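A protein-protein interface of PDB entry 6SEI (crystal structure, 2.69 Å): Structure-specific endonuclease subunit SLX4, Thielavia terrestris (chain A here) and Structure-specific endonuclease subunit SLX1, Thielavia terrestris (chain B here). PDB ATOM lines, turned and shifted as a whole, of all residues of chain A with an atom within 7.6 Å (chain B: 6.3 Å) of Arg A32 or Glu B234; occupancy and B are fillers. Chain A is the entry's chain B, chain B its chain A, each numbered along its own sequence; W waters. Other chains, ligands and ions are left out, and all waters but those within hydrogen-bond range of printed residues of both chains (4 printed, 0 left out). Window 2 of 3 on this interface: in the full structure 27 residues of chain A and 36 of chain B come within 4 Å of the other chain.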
ATOM      1  N   VAL A  28     -19.546  19.262  -1.648  1.00  0.00           N
ATOM      2  CA  VAL A  28     -19.419  18.930  -3.062  1.00  0.00           C
ATOM      3  C   VAL A  28     -19.816  20.101  -3.959  1.00  0.00           C
ATOM      4  O   VAL A  28     -19.206  20.316  -5.016  1.00  0.00           O
ATOM      5  CB  VAL A  28     -20.253  17.666  -3.356  1.00  0.00           C
ATOM      6  CG1 VAL A  28     -20.695  17.616  -4.803  1.00  0.00           C
ATOM      7  CG2 VAL A  28     -19.459  16.424  -2.999  1.00  0.00           C
ATOM      8  N   THR A  29     -20.822  20.879  -3.565  1.00  0.00           N
ATOM      9  CA  THR A  29     -21.382  21.912  -4.427  1.00  0.00           C
ATOM     10  C   THR A  29     -20.760  23.288  -4.215  1.00  0.00           C
ATOM     11  O   THR A  29     -21.158  24.241  -4.890  1.00  0.00           O
ATOM     12  CB  THR A  29     -22.899  22.002  -4.229  1.00  0.00           C
ATOM     13  OG1 THR A  29     -23.184  22.455  -2.900  1.00  0.00           O
ATOM     14  CG2 THR A  29     -23.547  20.644  -4.449  1.00  0.00           C
ATOM     15  N   ALA A  30     -19.805  23.421  -3.300  1.00  0.00           N
ATOM     16  CA  ALA A  30     -19.116  24.689  -3.154  1.00  0.00           C
ATOM     17  C   ALA A  30     -18.293  24.976  -4.409  1.00  0.00           C
ATOM     18  O   ALA A  30     -17.829  24.049  -5.079  1.00  0.00           O
ATOM     19  CB  ALA A  30     -18.213  24.671  -1.924  1.00  0.00           C
ATOM     20  N   PRO A  31     -18.115  26.253  -4.762  1.00  0.00           N
ATOM     21  CA  PRO A  31     -17.320  26.578  -5.954  1.00  0.00           C
ATOM     22  C   PRO A  31     -15.881  26.097  -5.821  1.00  0.00           C
ATOM     23  O   PRO A  31     -15.324  26.012  -4.724  1.00  0.00           O
ATOM     24  CB  PRO A  31     -17.400  28.109  -6.035  1.00  0.00           C
ATOM     25  CG  PRO A  31     -17.875  28.557  -4.696  1.00  0.00           C
ATOM     26  CD  PRO A  31     -18.733  27.451  -4.171  1.00  0.00           C
ATOM     27  N   ARG A  32     -15.286  25.772  -6.965  1.00  0.00           N
ATOM     28  CA  ARG A  32     -13.950  25.203  -6.995  1.00  0.00           C
ATOM     29  C   ARG A  32     -12.892  26.299  -6.908  1.00  0.00           C
ATOM     30  O   ARG A  32     -13.163  27.482  -7.127  1.00  0.00           O
ATOM     31  CB  ARG A  32     -13.750  24.379  -8.269  1.00  0.00           C
ATOM     32  CG  ARG A  32     -13.449  25.221  -9.496  1.00  0.00           C
ATOM     33  CD  ARG A  32     -13.830  24.516 -10.784  1.00  0.00           C
ATOM     34  NE  ARG A  32     -13.668  25.409 -11.927  1.00  0.00           N
ATOM     35  CZ  ARG A  32     -14.295  25.266 -13.090  1.00  0.00           C
ATOM     36  NH1 ARG A  32     -15.133  24.256 -13.282  1.00  0.00           N
ATOM     37  NH2 ARG A  32     -14.079  26.134 -14.067  1.00  0.00           N
ATOM     38  N   ALA A  33     -11.670  25.884  -6.586  1.00  0.00           N
ATOM     39  CA  ALA A  33     -10.574  26.830  -6.422  1.00  0.00           C
ATOM     40  C   ALA A  33     -10.232  27.504  -7.739  1.00  0.00           C
ATOM     41  O   ALA A  33     -10.110  26.844  -8.773  1.00  0.00           O
ATOM     42  CB  ALA A  33      -9.340  26.116  -5.878  1.00  0.00           C
ATOM     43  N   LYS A  34     -10.078  28.825  -7.698  1.00  0.00           N
ATOM     44  CA  LYS A  34      -9.499  29.555  -8.819  1.00  0.00           C
ATOM     45  C   LYS A  34      -7.984  29.627  -8.721  1.00  0.00           C
ATOM     46  O   LYS A  34      -7.302  29.711  -9.749  1.00  0.00           O
ATOM     47  CB  LYS A  34     -10.077  30.970  -8.893  1.00  0.00           C
ATOM     48  CG  LYS A  34     -11.589  31.011  -9.050  1.00  0.00           C
ATOM     49  CD  LYS A  34     -12.067  32.417  -9.356  1.00  0.00           C
ATOM     50  CE  LYS A  34     -13.588  32.496  -9.379  1.00  0.00           C
ATOM     51  NZ  LYS A  34     -14.134  32.554 -10.770  1.00  0.00           N
ATOM     52  N   ASP A  35      -7.450  29.594  -7.499  1.00  0.00           N
ATOM     53  CA  ASP A  35      -6.020  29.533  -7.256  1.00  0.00           C
ATOM     54  C   ASP A  35      -5.669  28.116  -6.828  1.00  0.00           C
ATOM     55  O   ASP A  35      -6.030  27.714  -5.712  1.00  0.00           O
ATOM     56  CB  ASP A  35      -5.622  30.534  -6.172  1.00  0.00           C
ATOM     57  CG  ASP A  35      -4.123  30.578  -5.925  1.00  0.00           C
ATOM     58  OD1 ASP A  35      -3.372  29.810  -6.563  1.00  0.00           O
ATOM     59  OD2 ASP A  35      -3.695  31.389  -5.080  1.00  0.00           O
ATOM     60  N   ASN A  38      -4.852  27.183  -3.361  1.00  0.00           N
ATOM     61  CA  ASN A  38      -5.885  27.340  -2.338  1.00  0.00           C
ATOM     62  C   ASN A  38      -7.105  26.512  -2.725  1.00  0.00           C
ATOM     63  O   ASN A  38      -8.148  27.057  -3.110  1.00  0.00           O
ATOM     64  CB  ASN A  38      -6.245  28.814  -2.158  1.00  0.00           C
ATOM     65  CG  ASN A  38      -7.052  29.063  -0.909  1.00  0.00           C
ATOM     66  OD1 ASN A  38      -6.587  28.817   0.204  1.00  0.00           O
ATOM     67  ND2 ASN A  38      -8.272  29.559  -1.083  1.00  0.00           N
ATOM     68  N   PRO A  39      -7.011  25.187  -2.616  1.00  0.00           N
ATOM     69  CA  PRO A  39      -8.124  24.332  -3.036  1.00  0.00           C
ATOM     70  C   PRO A  39      -9.283  24.394  -2.057  1.00  0.00           C
ATOM     71  O   PRO A  39      -9.113  24.672  -0.868  1.00  0.00           O
ATOM     72  CB  PRO A  39      -7.500  22.935  -3.060  1.00  0.00           C
ATOM     73  CG  PRO A  39      -6.447  22.998  -2.009  1.00  0.00           C
ATOM     74  CD  PRO A  39      -5.895  24.402  -2.055  1.00  0.00           C
ATOM     75  N   SER A  40     -10.478  24.129  -2.579  1.00  0.00           N
ATOM     76  CA  SER A  40     -11.651  24.004  -1.733  1.00  0.00           C
ATOM     77  C   SER A  40     -11.539  22.751  -0.870  1.00  0.00           C
ATOM     78  O   SER A  40     -10.701  21.876  -1.104  1.00  0.00           O
ATOM     79  CB  SER A  40     -12.919  23.952  -2.583  1.00  0.00           C
ATOM     80  OG  SER A  40     -13.061  22.685  -3.203  1.00  0.00           O
ATOM     81  N   HIS A  42     -13.479  20.280  -0.807  1.00  0.00           N
ATOM     82  CA  HIS A  42     -13.701  19.120  -1.662  1.00  0.00           C
ATOM     83  C   HIS A  42     -12.430  18.735  -2.404  1.00  0.00           C
ATOM     84  O   HIS A  42     -12.102  17.548  -2.517  1.00  0.00           O
ATOM     85  CB  HIS A  42     -14.834  19.414  -2.647  1.00  0.00           C
ATOM     86  CG  HIS A  42     -15.224  18.243  -3.495  1.00  0.00           C
ATOM     87  ND1 HIS A  42     -15.865  18.386  -4.708  1.00  0.00           N
ATOM     88  CD2 HIS A  42     -15.076  16.910  -3.305  1.00  0.00           C
ATOM     89  CE1 HIS A  42     -16.089  17.193  -5.230  1.00  0.00           C
ATOM     90  NE2 HIS A  42     -15.621  16.280  -4.398  1.00  0.00           N
ATOM     91  N   GLU A  43     -11.694  19.725  -2.910  1.00  0.00           N
ATOM     92  CA  GLU A  43     -10.475  19.424  -3.652  1.00  0.00           C
ATOM     93  C   GLU A  43      -9.352  18.979  -2.725  1.00  0.00           C
ATOM     94  O   GLU A  43      -8.457  18.239  -3.149  1.00  0.00           O
ATOM     95  CB  GLU A  43     -10.057  20.640  -4.479  1.00  0.00           C
ATOM     96  CG  GLU A  43     -11.030  20.956  -5.604  1.00  0.00           C
ATOM     97  CD  GLU A  43     -10.819  22.333  -6.202  1.00  0.00           C
ATOM     98  OE1 GLU A  43     -10.648  23.297  -5.425  1.00  0.00           O
ATOM     99  OE2 GLU A  43     -10.834  22.454  -7.448  1.00  0.00           O
ATOM    100  N   GLY B 227      -5.583  22.688 -23.314  1.00  0.00           N
ATOM    101  CA  GLY B 227      -6.816  22.786 -24.074  1.00  0.00           C
ATOM    102  C   GLY B 227      -8.013  22.984 -23.172  1.00  0.00           C
ATOM    103  O   GLY B 227      -8.054  23.908 -22.352  1.00  0.00           O
ATOM    104  N   ALA B 228      -9.004  22.107 -23.315  1.00  0.00           N
ATOM    105  CA  ALA B 228     -10.242  22.199 -22.557  1.00  0.00           C
ATOM    106  C   ALA B 228     -10.501  20.898 -21.809  1.00  0.00           C
ATOM    107  O   ALA B 228     -10.023  19.827 -22.196  1.00  0.00           O
ATOM    108  CB  ALA B 228     -11.435  22.528 -23.469  1.00  0.00           C
ATOM    109  N   CYS B 229     -11.262  21.009 -20.728  1.00  0.00           N
ATOM    110  CA  CYS B 229     -11.545  19.865 -19.877  1.00  0.00           C
ATOM    111  C   CYS B 229     -12.284  18.780 -20.647  1.00  0.00           C
ATOM    112  O   CYS B 229     -13.330  19.035 -21.256  1.00  0.00           O
ATOM    113  CB  CYS B 229     -12.369  20.330 -18.679  1.00  0.00           C
ATOM    114  SG  CYS B 229     -12.927  19.037 -17.557  1.00  0.00           S
ATOM    115  N   VAL B 230     -11.744  17.561 -20.589  1.00  0.00           N
ATOM    116  CA  VAL B 230     -12.309  16.437 -21.320  1.00  0.00           C
ATOM    117  C   VAL B 230     -13.691  16.051 -20.821  1.00  0.00           C
ATOM    118  O   VAL B 230     -14.394  15.298 -21.498  1.00  0.00           O
ATOM    119  CB  VAL B 230     -11.371  15.209 -21.255  1.00  0.00           C
ATOM    120  CG1 VAL B 230     -10.139  15.430 -22.117  1.00  0.00           C
ATOM    121  CG2 VAL B 230     -10.974  14.924 -19.814  1.00  0.00           C
ATOM    122  N   VAL B 231     -14.104  16.552 -19.660  1.00  0.00           N
ATOM    123  CA  VAL B 231     -15.407  16.215 -19.101  1.00  0.00           C
ATOM    124  C   VAL B 231     -16.422  17.313 -19.409  1.00  0.00           C
ATOM    125  O   VAL B 231     -17.406  17.075 -20.114  1.00  0.00           O
ATOM    126  CB  VAL B 231     -15.305  15.952 -17.586  1.00  0.00           C
ATOM    127  CG1 VAL B 231     -16.570  15.271 -17.084  1.00  0.00           C
ATOM    128  CG2 VAL B 231     -14.079  15.099 -17.272  1.00  0.00           C
ATOM    129  N   CYS B 232     -16.186  18.526 -18.898  1.00  0.00           N
ATOM    130  CA  CYS B 232     -17.156  19.615 -18.986  1.00  0.00           C
ATOM    131  C   CYS B 232     -17.030  20.453 -20.257  1.00  0.00           C
ATOM    132  O   CYS B 232     -17.885  21.317 -20.493  1.00  0.00           O
ATOM    133  CB  CYS B 232     -17.044  20.516 -17.746  1.00  0.00           C
ATOM    134  SG  CYS B 232     -15.674  21.672 -17.730  1.00  0.00           S
ATOM    135  N   ARG B 233     -15.995  20.228 -21.072  1.00  0.00           N
ATOM    136  CA  ARG B 233     -15.749  20.896 -22.351  1.00  0.00           C
ATOM    137  C   ARG B 233     -15.413  22.379 -22.216  1.00  0.00           C
ATOM    138  O   ARG B 233     -15.447  23.107 -23.217  1.00  0.00           O
ATOM    139  CB  ARG B 233     -16.931  20.746 -23.319  1.00  0.00           C
ATOM    140  CG  ARG B 233     -17.480  19.335 -23.466  1.00  0.00           C
ATOM    141  CD  ARG B 233     -18.302  19.209 -24.736  1.00  0.00           C
ATOM    142  NE  ARG B 233     -19.450  20.116 -24.743  1.00  0.00           N
ATOM    143  CZ  ARG B 233     -20.130  20.452 -25.836  1.00  0.00           C
ATOM    144  NH1 ARG B 233     -19.775  19.961 -27.015  1.00  0.00           N
ATOM    145  NH2 ARG B 233     -21.163  21.280 -25.754  1.00  0.00           N
ATOM    146  N   GLU B 234     -15.073  22.851 -21.022  1.00  0.00           N
ATOM    147  CA  GLU B 234     -14.764  24.259 -20.813  1.00  0.00           C
ATOM    148  C   GLU B 234     -13.266  24.499 -20.947  1.00  0.00           C
ATOM    149  O   GLU B 234     -12.455  23.722 -20.435  1.00  0.00           O
ATOM    150  CB  GLU B 234     -15.244  24.717 -19.436  1.00  0.00           C
ATOM    151  CG  GLU B 234     -14.704  26.070 -19.005  1.00  0.00           C
ATOM    152  CD  GLU B 234     -15.046  26.411 -17.568  1.00  0.00           C
ATOM    153  OE1 GLU B 234     -15.815  25.650 -16.939  1.00  0.00           O
ATOM    154  OE2 GLU B 234     -14.549  27.441 -17.064  1.00  0.00           O
ATOM    155  N   GLU B 235     -12.905  25.576 -21.644  1.00  0.00           N
ATOM    156  CA  GLU B 235     -11.504  25.955 -21.777  1.00  0.00           C
ATOM    157  C   GLU B 235     -10.856  26.107 -20.402  1.00  0.00           C
ATOM    158  O   GLU B 235     -11.495  26.506 -19.427  1.00  0.00           O
ATOM    159  CB  GLU B 235     -11.383  27.260 -22.567  1.00  0.00           C
ATOM    160  CG  GLU B 235     -11.917  28.491 -21.840  1.00  0.00           C
ATOM    161  CD  GLU B 235     -13.399  28.730 -22.089  1.00  0.00           C
ATOM    162  OE1 GLU B 235     -14.062  27.862 -22.700  1.00  0.00           O
ATOM    163  OE2 GLU B 235     -13.899  29.795 -21.674  1.00  0.00           O
ATOM    164  N   MET B 236      -9.571  25.762 -20.324  1.00  0.00           N
ATOM    165  CA  MET B 236      -8.812  25.824 -19.073  1.00  0.00           C
ATOM    166  C   MET B 236      -7.584  26.700 -19.296  1.00  0.00           C
ATOM    167  O   MET B 236      -6.546  26.221 -19.762  1.00  0.00           O
ATOM    168  CB  MET B 236      -8.423  24.431 -18.593  1.00  0.00           C
ATOM    169  CG  MET B 236      -9.585  23.457 -18.500  1.00  0.00           C
ATOM    170  SD  MET B 236      -9.068  21.859 -17.858  1.00  0.00           S
ATOM    171  CE  MET B 236      -8.174  21.247 -19.276  1.00  0.00           C
ATOM    172  N   ASP B 240      -5.833  28.493 -13.854  1.00  0.00           N
ATOM    173  CA  ASP B 240      -7.238  28.575 -13.450  1.00  0.00           C
ATOM    174  C   ASP B 240      -7.632  27.268 -12.769  1.00  0.00           C
ATOM    175  O   ASP B 240      -8.138  26.340 -13.402  1.00  0.00           O
ATOM    176  CB  ASP B 240      -8.125  28.872 -14.654  1.00  0.00           C
ATOM    177  CG  ASP B 240      -9.589  29.010 -14.282  1.00  0.00           C
ATOM    178  OD1 ASP B 240      -9.894  29.129 -13.075  1.00  0.00           O
ATOM    179  OD2 ASP B 240     -10.438  29.005 -15.198  1.00  0.00           O
ATOM    180  N   GLY B 241      -7.408  27.206 -11.459  1.00  0.00           N
ATOM    181  CA  GLY B 241      -7.787  26.048 -10.682  1.00  0.00           C
ATOM    182  C   GLY B 241      -6.855  24.868 -10.881  1.00  0.00           C
ATOM    183  O   GLY B 241      -5.813  24.943 -11.538  1.00  0.00           O
ATOM    184  N   HIS B 256     -10.769  19.480 -15.159  1.00  0.00           N
ATOM    185  CA  HIS B 256     -10.935  20.093 -13.848  1.00  0.00           C
ATOM    186  C   HIS B 256     -10.964  19.000 -12.789  1.00  0.00           C
ATOM    187  O   HIS B 256     -11.626  17.971 -12.969  1.00  0.00           O
ATOM    188  CB  HIS B 256     -12.216  20.920 -13.799  1.00  0.00           C
ATOM    189  CG  HIS B 256     -12.190  22.125 -14.684  1.00  0.00           C
ATOM    190  ND1 HIS B 256     -12.842  22.170 -15.897  1.00  0.00           N
ATOM    191  CD2 HIS B 256     -11.593  23.331 -14.533  1.00  0.00           C
ATOM    192  CE1 HIS B 256     -12.645  23.348 -16.458  1.00  0.00           C
ATOM    193  NE2 HIS B 256     -11.889  24.073 -15.651  1.00  0.00           N
ATOM    194  N   SER B 258     -12.362  18.475  -9.961  1.00  0.00           N
ATOM    195  CA  SER B 258     -13.688  18.033  -9.552  1.00  0.00           C
ATOM    196  C   SER B 258     -14.548  17.561 -10.716  1.00  0.00           C
ATOM    197  O   SER B 258     -15.618  16.999 -10.476  1.00  0.00           O
ATOM    198  CB  SER B 258     -14.411  19.150  -8.793  1.00  0.00           C
ATOM    199  OG  SER B 258     -14.482  20.335  -9.565  1.00  0.00           O
ATOM    200  N   CYS B 259     -14.120  17.763 -11.960  1.00  0.00           N
ATOM    201  CA  CYS B 259     -14.841  17.121 -13.051  1.00  0.00           C
ATOM    202  C   CYS B 259     -14.381  15.673 -13.218  1.00  0.00           C
ATOM    203  O   CYS B 259     -15.211  14.773 -13.379  1.00  0.00           O
ATOM    204  CB  CYS B 259     -14.694  17.924 -14.341  1.00  0.00           C
ATOM    205  SG  CYS B 259     -15.669  19.463 -14.364  1.00  0.00           S
HETATM  206  O   HOH W   1     -11.789  21.214  -9.379  1.00  0.00           O
HETATM  207  O   HOH W   2     -11.602  27.570 -11.853  1.00  0.00           O
HETATM  208  O   HOH W   3     -13.120  28.772 -14.421  1.00  0.00           O
HETATM  209  O   HOH W   4     -17.050  23.522 -15.839  1.00  0.00           O
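A ring nitrogen (NE2) of His B256 lies within hydrogen-bond range of the guanidinium group (NH2) of Arg A32, at 3.4 Å. OE2 of Glu B234 lies within salt-bridge range of NH2 of Arg A32 (3.3 Å). The backbone carbonyl oxygen of Lys A34 is in hydrogen-bond range of the backbone NH of Gly B241 (3.0 Å).
N of Cys B229 is in hydrogen-bond range of O of Glu B234 (3.0 Å). The backbone NH (N) of Glu B234 sits close to the side-chain sulfur (SG) of Cys B232 (3.5 Å). The side-chain carboxylate (OE1) of Glu A43 sits at hydrogen-bond distance from the backbone NH (N) of Ala A33, at 3.0 Å.
Ala A33 touches Gly B241. Lys A34 touches Asp B240 (O to CA, 3.9 Å).
Of chain B, only Glu B234 (3.3 Å) and His B256 (3.4 Å) come within 4 Å of Arg A32. Printed residues of chain B within 4 Å of Ala A33: Gly B241 (3.1 Å). Of the printed residues of chain B, Lys A34 touches Asp B240 (3.9 Å) and Gly B241 (3.0 Å). Asn A38 touches none of the printed residues of chain B. Of the printed residues of chain A, Glu B234 touches Arg A32 (3.3 Å). Of the printed residues of chain A, Asp B240 touches Lys A34 (3.9 Å). Of the printed residues of chain A, Gly B241 touches Ala A33 and Lys A34. Of the printed residues of chain A, His B256 touches Arg A32. The nearest printed residue of chain A that does not touch Glu B234 is Lys A34 (8.1 Å). The nearest printed residue of chain A that does not touch Gly B241 is Asp A35 (4.6 Å).
Printed residues of chain A that touch a printed residue of chain B: Arg A32, Ala A33 and Lys A34. Hydrophobic or aromatic side chains of chain B within 4 Å of the printed part of chain A: His B256. Among the printed residues, 5 pairs touch across the chains. Among the printed residues, Asp or Glu carboxylates within 4 Å of a Lys or Arg side-chain nitrogen of the other chain: Arg A32 with Glu B234.
Water W1 bridges the side-chain carboxylate (OE2) of Glu A43 and the side-chain hydroxyl (OG) of Ser B258. Water W2 lies within hydrogen-bond range of OD1 of Asp B240, NE of Arg A32 and O of Ala A33. Water W4 bridges OE1 of Glu B234 (2.7 Å) and NH1 of Arg A32 (3.3 Å). Water W3 lies within hydrogen-bond range of the side-chain carboxylate (OD2) of Asp B240, the guanidinium group (NH2) of Arg A32 and the side-chain carboxylate (OE2) of Glu B234.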
